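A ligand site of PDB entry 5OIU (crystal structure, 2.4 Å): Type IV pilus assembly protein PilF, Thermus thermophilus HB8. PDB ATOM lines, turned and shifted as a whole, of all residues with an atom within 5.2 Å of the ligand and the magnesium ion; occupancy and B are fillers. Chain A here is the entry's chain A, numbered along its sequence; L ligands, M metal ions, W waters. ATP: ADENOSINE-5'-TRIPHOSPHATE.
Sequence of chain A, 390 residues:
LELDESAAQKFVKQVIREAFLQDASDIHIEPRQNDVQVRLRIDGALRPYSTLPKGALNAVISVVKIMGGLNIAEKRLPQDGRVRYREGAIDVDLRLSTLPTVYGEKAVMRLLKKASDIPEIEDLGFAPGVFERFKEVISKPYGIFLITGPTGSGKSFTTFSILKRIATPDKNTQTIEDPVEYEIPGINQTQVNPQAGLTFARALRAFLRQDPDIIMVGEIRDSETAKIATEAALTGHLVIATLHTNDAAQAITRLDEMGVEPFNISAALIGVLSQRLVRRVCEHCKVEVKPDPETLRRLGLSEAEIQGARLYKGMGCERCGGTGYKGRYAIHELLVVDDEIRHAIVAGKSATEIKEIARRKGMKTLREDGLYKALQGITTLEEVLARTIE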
ATOM      1  N   ASP A  23      -1.703  15.784  11.417  1.00  0.00           N
ATOM      2  CA  ASP A  23      -3.033  16.315  11.105  1.00  0.00           C
ATOM      3  C   ASP A  23      -3.571  17.177  12.257  1.00  0.00           C
ATOM      4  O   ASP A  23      -4.740  17.061  12.646  1.00  0.00           O
ATOM      5  CB  ASP A  23      -4.026  15.203  10.736  1.00  0.00           C
ATOM      6  CG  ASP A  23      -5.314  15.737  10.037  1.00  0.00           C
ATOM      7  OD1 ASP A  23      -5.356  16.900   9.565  1.00  0.00           O
ATOM      8  OD2 ASP A  23      -6.281  14.970   9.911  1.00  0.00           O
ATOM      9  N   ARG A 110      -4.266  28.205  11.439  1.00  0.00           N
ATOM     10  CA  ARG A 110      -5.182  27.130  11.092  1.00  0.00           C
ATOM     11  C   ARG A 110      -4.754  26.481   9.784  1.00  0.00           C
ATOM     12  O   ARG A 110      -4.734  27.144   8.738  1.00  0.00           O
ATOM     13  CB  ARG A 110      -6.615  27.636  10.944  1.00  0.00           C
ATOM     14  CG  ARG A 110      -7.561  26.472  10.638  1.00  0.00           C
ATOM     15  CD  ARG A 110      -9.005  26.764  10.927  1.00  0.00           C
ATOM     16  NE  ARG A 110      -9.281  26.804  12.344  1.00  0.00           N
ATOM     17  CZ  ARG A 110     -10.494  26.928  12.861  1.00  0.00           C
ATOM     18  NH1 ARG A 110     -11.559  26.994  12.057  1.00  0.00           N
ATOM     19  NH2 ARG A 110     -10.651  26.946  14.183  1.00  0.00           N
ATOM     20  N   LYS A 113      -7.811  22.743   4.769  1.00  0.00           N
ATOM     21  CA  LYS A 113      -7.987  21.565   3.931  1.00  0.00           C
ATOM     22  C   LYS A 113      -8.097  21.960   2.451  1.00  0.00           C
ATOM     23  O   LYS A 113      -8.318  23.121   2.107  1.00  0.00           O
ATOM     24  CB  LYS A 113      -9.222  20.778   4.357  1.00  0.00           C
ATOM     25  CG  LYS A 113      -9.159  20.130   5.728  1.00  0.00           C
ATOM     26  CD  LYS A 113      -7.858  19.384   5.928  1.00  0.00           C
ATOM     27  CE  LYS A 113      -8.059  18.190   6.851  1.00  0.00           C
ATOM     28  NZ  LYS A 113      -6.773  17.569   7.229  1.00  0.00           N
ATOM     29  N   ASP A 123     -17.809   7.505   1.875  1.00  0.00           N
ATOM     30  CA  ASP A 123     -16.828   7.525   2.950  1.00  0.00           C
ATOM     31  C   ASP A 123     -17.137   8.574   4.023  1.00  0.00           C
ATOM     32  O   ASP A 123     -16.240   8.969   4.780  1.00  0.00           O
ATOM     33  CB  ASP A 123     -15.427   7.768   2.378  1.00  0.00           C
ATOM     34  CG  ASP A 123     -15.117   6.830   1.214  1.00  0.00           C
ATOM     35  OD1 ASP A 123     -15.348   5.603   1.354  1.00  0.00           O
ATOM     36  OD2 ASP A 123     -14.632   7.320   0.158  1.00  0.00           O
ATOM     37  N   LEU A 124     -18.384   9.045   4.107  1.00  0.00           N
ATOM     38  CA  LEU A 124     -18.742  10.047   5.099  1.00  0.00           C
ATOM     39  C   LEU A 124     -19.055   9.427   6.456  1.00  0.00           C
ATOM     40  O   LEU A 124     -19.233  10.167   7.424  1.00  0.00           O
ATOM     41  CB  LEU A 124     -19.940  10.877   4.647  1.00  0.00           C
ATOM     42  CG  LEU A 124     -19.780  11.933   3.543  1.00  0.00           C
ATOM     43  CD1 LEU A 124     -21.153  12.474   3.135  1.00  0.00           C
ATOM     44  CD2 LEU A 124     -18.872  13.074   3.973  1.00  0.00           C
ATOM     45  N   PRO A 150     -22.924  22.417  15.373  1.00  0.00           N
ATOM     46  CA  PRO A 150     -22.007  23.428  15.905  1.00  0.00           C
ATOM     47  C   PRO A 150     -20.695  23.480  15.126  1.00  0.00           C
ATOM     48  O   PRO A 150     -20.500  22.675  14.200  1.00  0.00           O
ATOM     49  CB  PRO A 150     -21.769  22.984  17.348  1.00  0.00           C
ATOM     50  CG  PRO A 150     -22.199  21.553  17.402  1.00  0.00           C
ATOM     51  CD  PRO A 150     -23.208  21.330  16.339  1.00  0.00           C
ATOM     52  N   THR A 151     -19.807  24.405  15.484  1.00  0.00           N
ATOM     53  CA  THR A 151     -18.580  24.588  14.720  1.00  0.00           C
ATOM     54  C   THR A 151     -17.739  23.321  14.727  1.00  0.00           C
ATOM     55  O   THR A 151     -17.740  22.538  15.689  1.00  0.00           O
ATOM     56  CB  THR A 151     -17.780  25.777  15.267  1.00  0.00           C
ATOM     57  OG1 THR A 151     -16.648  26.046  14.425  1.00  0.00           O
ATOM     58  CG2 THR A 151     -17.300  25.469  16.682  1.00  0.00           C
ATOM     59  N   GLY A 152     -17.043  23.074  13.610  1.00  0.00           N
ATOM     60  CA  GLY A 152     -16.166  21.925  13.494  1.00  0.00           C
ATOM     61  C   GLY A 152     -16.837  20.575  13.609  1.00  0.00           C
ATOM     62  O   GLY A 152     -16.247  19.638  14.157  1.00  0.00           O
ATOM     63  N   SER A 153     -18.055  20.445  13.119  1.00  0.00           N
ATOM     64  CA  SER A 153     -18.708  19.140  13.101  1.00  0.00           C
ATOM     65  C   SER A 153     -18.712  18.512  11.722  1.00  0.00           C
ATOM     66  O   SER A 153     -19.440  17.539  11.500  1.00  0.00           O
ATOM     67  CB  SER A 153     -20.130  19.255  13.629  1.00  0.00           C
ATOM     68  OG  SER A 153     -20.846  20.238  12.915  1.00  0.00           O
ATOM     69  N   GLY A 154     -17.919  19.033  10.783  1.00  0.00           N
ATOM     70  CA  GLY A 154     -17.808  18.444   9.457  1.00  0.00           C
ATOM     71  C   GLY A 154     -18.817  18.916   8.446  1.00  0.00           C
ATOM     72  O   GLY A 154     -18.925  18.292   7.374  1.00  0.00           O
ATOM     73  N   LYS A 155     -19.559  19.993   8.711  1.00  0.00           N
ATOM     74  CA  LYS A 155     -20.655  20.355   7.825  1.00  0.00           C
ATOM     75  C   LYS A 155     -20.157  20.654   6.425  1.00  0.00           C
ATOM     76  O   LYS A 155     -20.739  20.173   5.437  1.00  0.00           O
ATOM     77  CB  LYS A 155     -21.435  21.525   8.411  1.00  0.00           C
ATOM     78  CG  LYS A 155     -21.915  21.264   9.850  1.00  0.00           C
ATOM     79  CD  LYS A 155     -22.962  22.293  10.279  1.00  0.00           C
ATOM     80  CE  LYS A 155     -22.344  23.663  10.441  1.00  0.00           C
ATOM     81  NZ  LYS A 155     -21.337  23.703  11.525  1.00  0.00           N
ATOM     82  N   SER A 156     -19.036  21.394   6.300  1.00  0.00           N
ATOM     83  CA  SER A 156     -18.510  21.742   4.976  1.00  0.00           C
ATOM     84  C   SER A 156     -18.085  20.497   4.203  1.00  0.00           C
ATOM     85  O   SER A 156     -18.305  20.414   2.984  1.00  0.00           O
ATOM     86  CB  SER A 156     -17.340  22.730   5.099  1.00  0.00           C
ATOM     87  OG  SER A 156     -17.755  24.025   5.526  1.00  0.00           O
ATOM     88  N   PHE A 157     -17.451  19.524   4.874  1.00  0.00           N
ATOM     89  CA  PHE A 157     -17.053  18.297   4.190  1.00  0.00           C
ATOM     90  C   PHE A 157     -18.275  17.606   3.597  1.00  0.00           C
ATOM     91  O   PHE A 157     -18.308  17.283   2.401  1.00  0.00           O
ATOM     92  CB  PHE A 157     -16.314  17.346   5.146  1.00  0.00           C
ATOM     93  CG  PHE A 157     -14.804  17.480   5.111  1.00  0.00           C
ATOM     94  CD1 PHE A 157     -14.212  18.732   5.095  1.00  0.00           C
ATOM     95  CD2 PHE A 157     -13.981  16.365   5.130  1.00  0.00           C
ATOM     96  CE1 PHE A 157     -12.824  18.866   5.075  1.00  0.00           C
ATOM     97  CE2 PHE A 157     -12.597  16.487   5.104  1.00  0.00           C
ATOM     98  CZ  PHE A 157     -12.012  17.725   5.072  1.00  0.00           C
ATOM     99  N   THR A 158     -19.297  17.388   4.416  1.00  0.00           N
ATOM    100  CA  THR A 158     -20.538  16.841   3.881  1.00  0.00           C
ATOM    101  C   THR A 158     -21.011  17.645   2.679  1.00  0.00           C
ATOM    102  O   THR A 158     -21.171  17.095   1.583  1.00  0.00           O
ATOM    103  CB  THR A 158     -21.590  16.800   4.987  1.00  0.00           C
ATOM    104  OG1 THR A 158     -21.059  16.043   6.087  1.00  0.00           O
ATOM    105  CG2 THR A 158     -22.873  16.164   4.528  1.00  0.00           C
ATOM    106  N   GLU A 181     -13.581  28.172   0.769  1.00  0.00           N
ATOM    107  CA  GLU A 181     -12.627  27.332   1.477  1.00  0.00           C
ATOM    108  C   GLU A 181     -11.761  26.542   0.490  1.00  0.00           C
ATOM    109  O   GLU A 181     -10.541  26.688   0.463  1.00  0.00           O
ATOM    110  CB  GLU A 181     -13.373  26.395   2.446  1.00  0.00           C
ATOM    111  CG  GLU A 181     -14.215  27.151   3.477  1.00  0.00           C
ATOM    112  CD  GLU A 181     -14.876  26.241   4.512  1.00  0.00           C
ATOM    113  OE1 GLU A 181     -14.211  25.276   4.959  1.00  0.00           O
ATOM    114  OE2 GLU A 181     -16.046  26.514   4.907  1.00  0.00           O
ATOM    115  N   TYR A 182     -12.385  25.698  -0.316  1.00  0.00           N
ATOM    116  CA  TYR A 182     -11.667  24.898  -1.300  1.00  0.00           C
ATOM    117  C   TYR A 182     -11.969  25.428  -2.691  1.00  0.00           C
ATOM    118  O   TYR A 182     -12.984  26.081  -2.931  1.00  0.00           O
ATOM    119  CB  TYR A 182     -12.068  23.420  -1.213  1.00  0.00           C
ATOM    120  CG  TYR A 182     -12.514  23.035   0.171  1.00  0.00           C
ATOM    121  CD1 TYR A 182     -11.596  22.941   1.216  1.00  0.00           C
ATOM    122  CD2 TYR A 182     -13.854  22.794   0.437  1.00  0.00           C
ATOM    123  CE1 TYR A 182     -12.006  22.605   2.492  1.00  0.00           C
ATOM    124  CE2 TYR A 182     -14.274  22.450   1.717  1.00  0.00           C
ATOM    125  CZ  TYR A 182     -13.342  22.358   2.737  1.00  0.00           C
ATOM    126  OH  TYR A 182     -13.749  22.024   4.022  1.00  0.00           O
ATOM    127  N   HIS A 244     -27.117  26.389  12.363  1.00  0.00           N
ATOM    128  CA  HIS A 244     -26.639  25.973  13.687  1.00  0.00           C
ATOM    129  C   HIS A 244     -27.847  25.685  14.576  1.00  0.00           C
ATOM    130  O   HIS A 244     -28.487  26.614  15.080  1.00  0.00           O
ATOM    131  CB  HIS A 244     -25.761  27.046  14.312  1.00  0.00           C
ATOM    132  CG  HIS A 244     -24.563  27.397  13.496  1.00  0.00           C
ATOM    133  ND1 HIS A 244     -23.639  26.455  13.094  1.00  0.00           N
ATOM    134  CD2 HIS A 244     -24.147  28.581  12.992  1.00  0.00           C
ATOM    135  CE1 HIS A 244     -22.692  27.048  12.380  1.00  0.00           C
ATOM    136  NE2 HIS A 244     -22.979  28.343  12.301  1.00  0.00           N
ATOM    137  N   GLN A 275     -25.348  16.659  12.437  1.00  0.00           N
ATOM    138  CA  GLN A 275     -24.176  15.811  12.538  1.00  0.00           C
ATOM    139  C   GLN A 275     -23.148  16.383  13.513  1.00  0.00           C
ATOM    140  O   GLN A 275     -23.108  17.597  13.763  1.00  0.00           O
ATOM    141  CB  GLN A 275     -23.552  15.593  11.147  1.00  0.00           C
ATOM    142  CG  GLN A 275     -22.384  16.500  10.819  1.00  0.00           C
ATOM    143  CD  GLN A 275     -21.733  16.181   9.454  1.00  0.00           C
ATOM    144  OE1 GLN A 275     -22.366  15.579   8.573  1.00  0.00           O
ATOM    145  NE2 GLN A 275     -20.488  16.617   9.277  1.00  0.00           N
ATOM    146  N   LEU A 277     -18.870  15.304  15.056  1.00  0.00           N
ATOM    147  CA  LEU A 277     -17.679  14.464  14.968  1.00  0.00           C
ATOM    148  C   LEU A 277     -17.342  13.994  16.367  1.00  0.00           C
ATOM    149  O   LEU A 277     -17.281  14.807  17.302  1.00  0.00           O
ATOM    150  CB  LEU A 277     -16.488  15.198  14.364  1.00  0.00           C
ATOM    151  CG  LEU A 277     -16.676  15.739  12.959  1.00  0.00           C
ATOM    152  CD1 LEU A 277     -15.477  16.544  12.539  1.00  0.00           C
ATOM    153  CD2 LEU A 277     -16.962  14.626  11.957  1.00  0.00           C
ATOM    154  N   ARG A 328     -11.209  11.179  13.941  1.00  0.00           N
ATOM    155  CA  ARG A 328     -12.578  11.552  14.253  1.00  0.00           C
ATOM    156  C   ARG A 328     -13.524  10.796  13.339  1.00  0.00           C
ATOM    157  O   ARG A 328     -13.165  10.372  12.244  1.00  0.00           O
ATOM    158  CB  ARG A 328     -12.768  13.063  14.170  1.00  0.00           C
ATOM    159  CG  ARG A 328     -12.262  13.741  15.455  1.00  0.00           C
ATOM    160  CD  ARG A 328     -12.434  15.240  15.455  1.00  0.00           C
ATOM    161  NE  ARG A 328     -11.650  15.891  14.413  1.00  0.00           N
ATOM    162  CZ  ARG A 328     -11.709  17.194  14.137  1.00  0.00           C
ATOM    163  NH1 ARG A 328     -12.528  17.968  14.858  1.00  0.00           N
ATOM    164  NH2 ARG A 328     -10.978  17.731  13.148  1.00  0.00           N
ATOM    165  N   TYR A 329     -14.738  10.598  13.825  1.00  0.00           N
ATOM    166  CA  TYR A 329     -15.742   9.893  13.066  1.00  0.00           C
ATOM    167  C   TYR A 329     -17.030  10.697  13.126  1.00  0.00           C
ATOM    168  O   TYR A 329     -17.335  11.314  14.150  1.00  0.00           O
ATOM    169  CB  TYR A 329     -15.957   8.506  13.622  1.00  0.00           C
ATOM    170  CG  TYR A 329     -16.387   7.480  12.599  1.00  0.00           C
ATOM    171  CD1 TYR A 329     -17.721   7.391  12.198  1.00  0.00           C
ATOM    172  CD2 TYR A 329     -15.475   6.604  12.046  1.00  0.00           C
ATOM    173  CE1 TYR A 329     -18.119   6.444  11.286  1.00  0.00           C
ATOM    174  CE2 TYR A 329     -15.861   5.657  11.141  1.00  0.00           C
ATOM    175  CZ  TYR A 329     -17.185   5.584  10.765  1.00  0.00           C
ATOM    176  OH  TYR A 329     -17.572   4.644   9.848  1.00  0.00           O
ATOM    177  N   ALA A 330     -17.780  10.692  12.033  1.00  0.00           N
ATOM    178  CA  ALA A 330     -19.014  11.463  12.001  1.00  0.00           C
ATOM    179  C   ALA A 330     -20.176  10.591  12.458  1.00  0.00           C
ATOM    180  O   ALA A 330     -20.208   9.399  12.179  1.00  0.00           O
ATOM    181  CB  ALA A 330     -19.264  12.022  10.588  1.00  0.00           C
HETATM  182  PG  ATP L   1     -16.902  25.316  10.560  1.00  0.00           P
HETATM  183  O1G ATP L   1     -17.919  25.481  11.672  1.00  0.00           O
HETATM  184  O2G ATP L   1     -15.547  25.935  10.767  1.00  0.00           O
HETATM  185  O3G ATP L   1     -17.408  25.596   9.148  1.00  0.00           O
HETATM  186  PB  ATP L   1     -17.502  22.624   9.782  1.00  0.00           P
HETATM  187  O1B ATP L   1     -18.739  22.147  10.500  1.00  0.00           O
HETATM  188  O2B ATP L   1     -17.623  23.126   8.345  1.00  0.00           O
HETATM  189  O3B ATP L   1     -16.646  23.711  10.602  1.00  0.00           O
HETATM  190  PA  ATP L   1     -15.657  20.970   8.550  1.00  0.00           P
HETATM  191  O1A ATP L   1     -16.497  20.398   7.445  1.00  0.00           O
HETATM  192  O2A ATP L   1     -14.787  22.158   8.180  1.00  0.00           O
HETATM  193  O3A ATP L   1     -16.492  21.374   9.864  1.00  0.00           O
HETATM  194  O5' ATP L   1     -14.763  19.790   9.173  1.00  0.00           O
HETATM  195  C5' ATP L   1     -13.891  20.090  10.257  1.00  0.00           C
HETATM  196  C4' ATP L   1     -12.796  19.063  10.241  1.00  0.00           C
HETATM  197  O4' ATP L   1     -13.336  17.833  10.706  1.00  0.00           O
HETATM  198  C3' ATP L   1     -12.312  18.806   8.825  1.00  0.00           C
HETATM  199  O3' ATP L   1     -11.141  19.569   8.583  1.00  0.00           O
HETATM  200  C2' ATP L   1     -11.915  17.372   8.872  1.00  0.00           C
HETATM  201  O2' ATP L   1     -10.615  17.330   9.463  1.00  0.00           O
HETATM  202  C1' ATP L   1     -12.844  16.757   9.895  1.00  0.00           C
HETATM  203  N9  ATP L   1     -14.003  16.074   9.250  1.00  0.00           N
HETATM  204  C8  ATP L   1     -14.980  16.664   8.534  1.00  0.00           C
HETATM  205  N7  ATP L   1     -15.883  15.752   8.102  1.00  0.00           N
HETATM  206  C5  ATP L   1     -15.498  14.536   8.561  1.00  0.00           C
HETATM  207  C6  ATP L   1     -16.007  13.141   8.479  1.00  0.00           C
HETATM  208  N6  ATP L   1     -17.152  12.823   7.799  1.00  0.00           N
HETATM  209  N1  ATP L   1     -15.291  12.173   9.094  1.00  0.00           N
HETATM  210  C2  ATP L   1     -14.165  12.495   9.779  1.00  0.00           C
HETATM  211  N3  ATP L   1     -13.639  13.739   9.891  1.00  0.00           N
HETATM  212  C4  ATP L   1     -14.256  14.778   9.317  1.00  0.00           C
HETATM  213 MG    MG M   1     -17.934  25.272   7.349  1.00  0.00          MG
HETATM  214  O   HOH W   1     -16.762  28.861   9.021  1.00  0.00           O
HETATM  215  O   HOH W   2     -14.614  27.506   8.346  1.00  0.00           O
HETATM  216  O   HOH W   3     -13.240  24.033  10.088  1.00  0.00           O
HETATM  217  O   HOH W   4     -15.895  24.745   7.506  1.00  0.00           O
HETATM  218  O   HOH W   5     -19.908  25.134   7.551  1.00  0.00           O
HETATM  219  O   HOH W   6     -18.545  15.121   7.105  1.00  0.00           O
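The magnesium ion is bound by an oxygen (O3G) of the ligand (1.9 Å), water W5 (2.0 Å), water W4 (2.1 Å), the side-chain hydroxyl of Ser 156 (2.2 Å) and an oxygen (O2B) of the ligand (2.4 Å). The magnesium ion has five donor atoms within binding distance.
The backbone NH of Ser 156 sits at hydrogen-bond distance from an oxygen (O1A) of the ligand (3.0 Å). N of Phe 157 sits at hydrogen-bond distance from O1A of the ligand, at 2.9 Å. The backbone NH (N) of Gly 154 is in hydrogen-bond range of an oxygen (O3A) of the ligand, 2.9 Å away. The backbone NH (N) of Lys 155 sits at hydrogen-bond distance from an oxygen (O1B) of the ligand (2.9 Å). NZ of Lys 155 lies within salt-bridge range of O1B of the ligand (3.2 Å). The side-chain hydroxyl (OG1) of Thr 151 sits at hydrogen-bond distance from an oxygen (O1G) of the ligand. The backbone NH (N) of Gly 152 lies within hydrogen-bond range of an oxygen (O3B) of the ligand, 3.1 Å away. N of Ser 153 lies within hydrogen-bond range of O1B of the ligand (3.2 Å). N6 of the ligand lies within hydrogen-bond range of O of Leu 124 (3.4 Å). The guanidinium group (NH2) of Arg 328 is in hydrogen-bond range of an oxygen (O4') of the ligand (3.4 Å).
CG of Lys 113 touches O3' of the ligand, at 3.5 Å. Leu 277 touches the ligand. Ala 330 touches the ligand (CB to N6, 3.6 Å). Hydrophobic or aromatic side chains that line the ligand: Phe 157, Leu 277 and Ala 330. The nearest printed residue that does not touch the ligand is Pro 150 (4.1 Å).
Water W4 bridges O2A of the ligand and OE1 of Glu 181. Water W6 lies within hydrogen-bond range of a nitrogen (N6) of the ligand (2.8 Å), the side-chain hydroxyl (OG1) of Thr 158 (2.9 Å), the backbone carbonyl oxygen (O) of Gly 154 (3.2 Å) and the side-chain amide nitrogen (NE2) of Gln 275 (3.3 Å).
OE2 of Glu 181 touches the magnesium ion, at 3.3 Å. Of the 22 residues printed, 2 come within 4 Å of the magnesium ion.
The side-chain hydroxyl of Ser 156 sits close to the side-chain carboxylate of Glu 181 (3.1 Å). The backbone carbonyl oxygen of Gly 154 sits close to the side-chain amide nitrogen of Gln 275, at 3.0 Å. OG1 of Thr 158 sits at hydrogen-bond distance from O of Gly 154 (3.4 Å). The backbone carbonyl oxygen (O) of Pro 150 is in hydrogen-bond range of the side-chain amino group (NZ) of Lys 155 (3.0 Å). O of Pro 150 sits at hydrogen-bond distance from OG of Ser 153 (2.8 Å). The backbone carbonyl oxygen (O) of Ser 153 is in hydrogen-bond range of the side-chain amide nitrogen (NE2) of Gln 275. The side-chain hydroxyl (OH) of Tyr 182 is in hydrogen-bond range of the side-chain carboxylate (OE1) of Glu 181, 3.4 Å away. The side-chain carboxylate (OD1) of Asp 23 lies within salt-bridge range of the side-chain amino group (NZ) of Lys 113.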
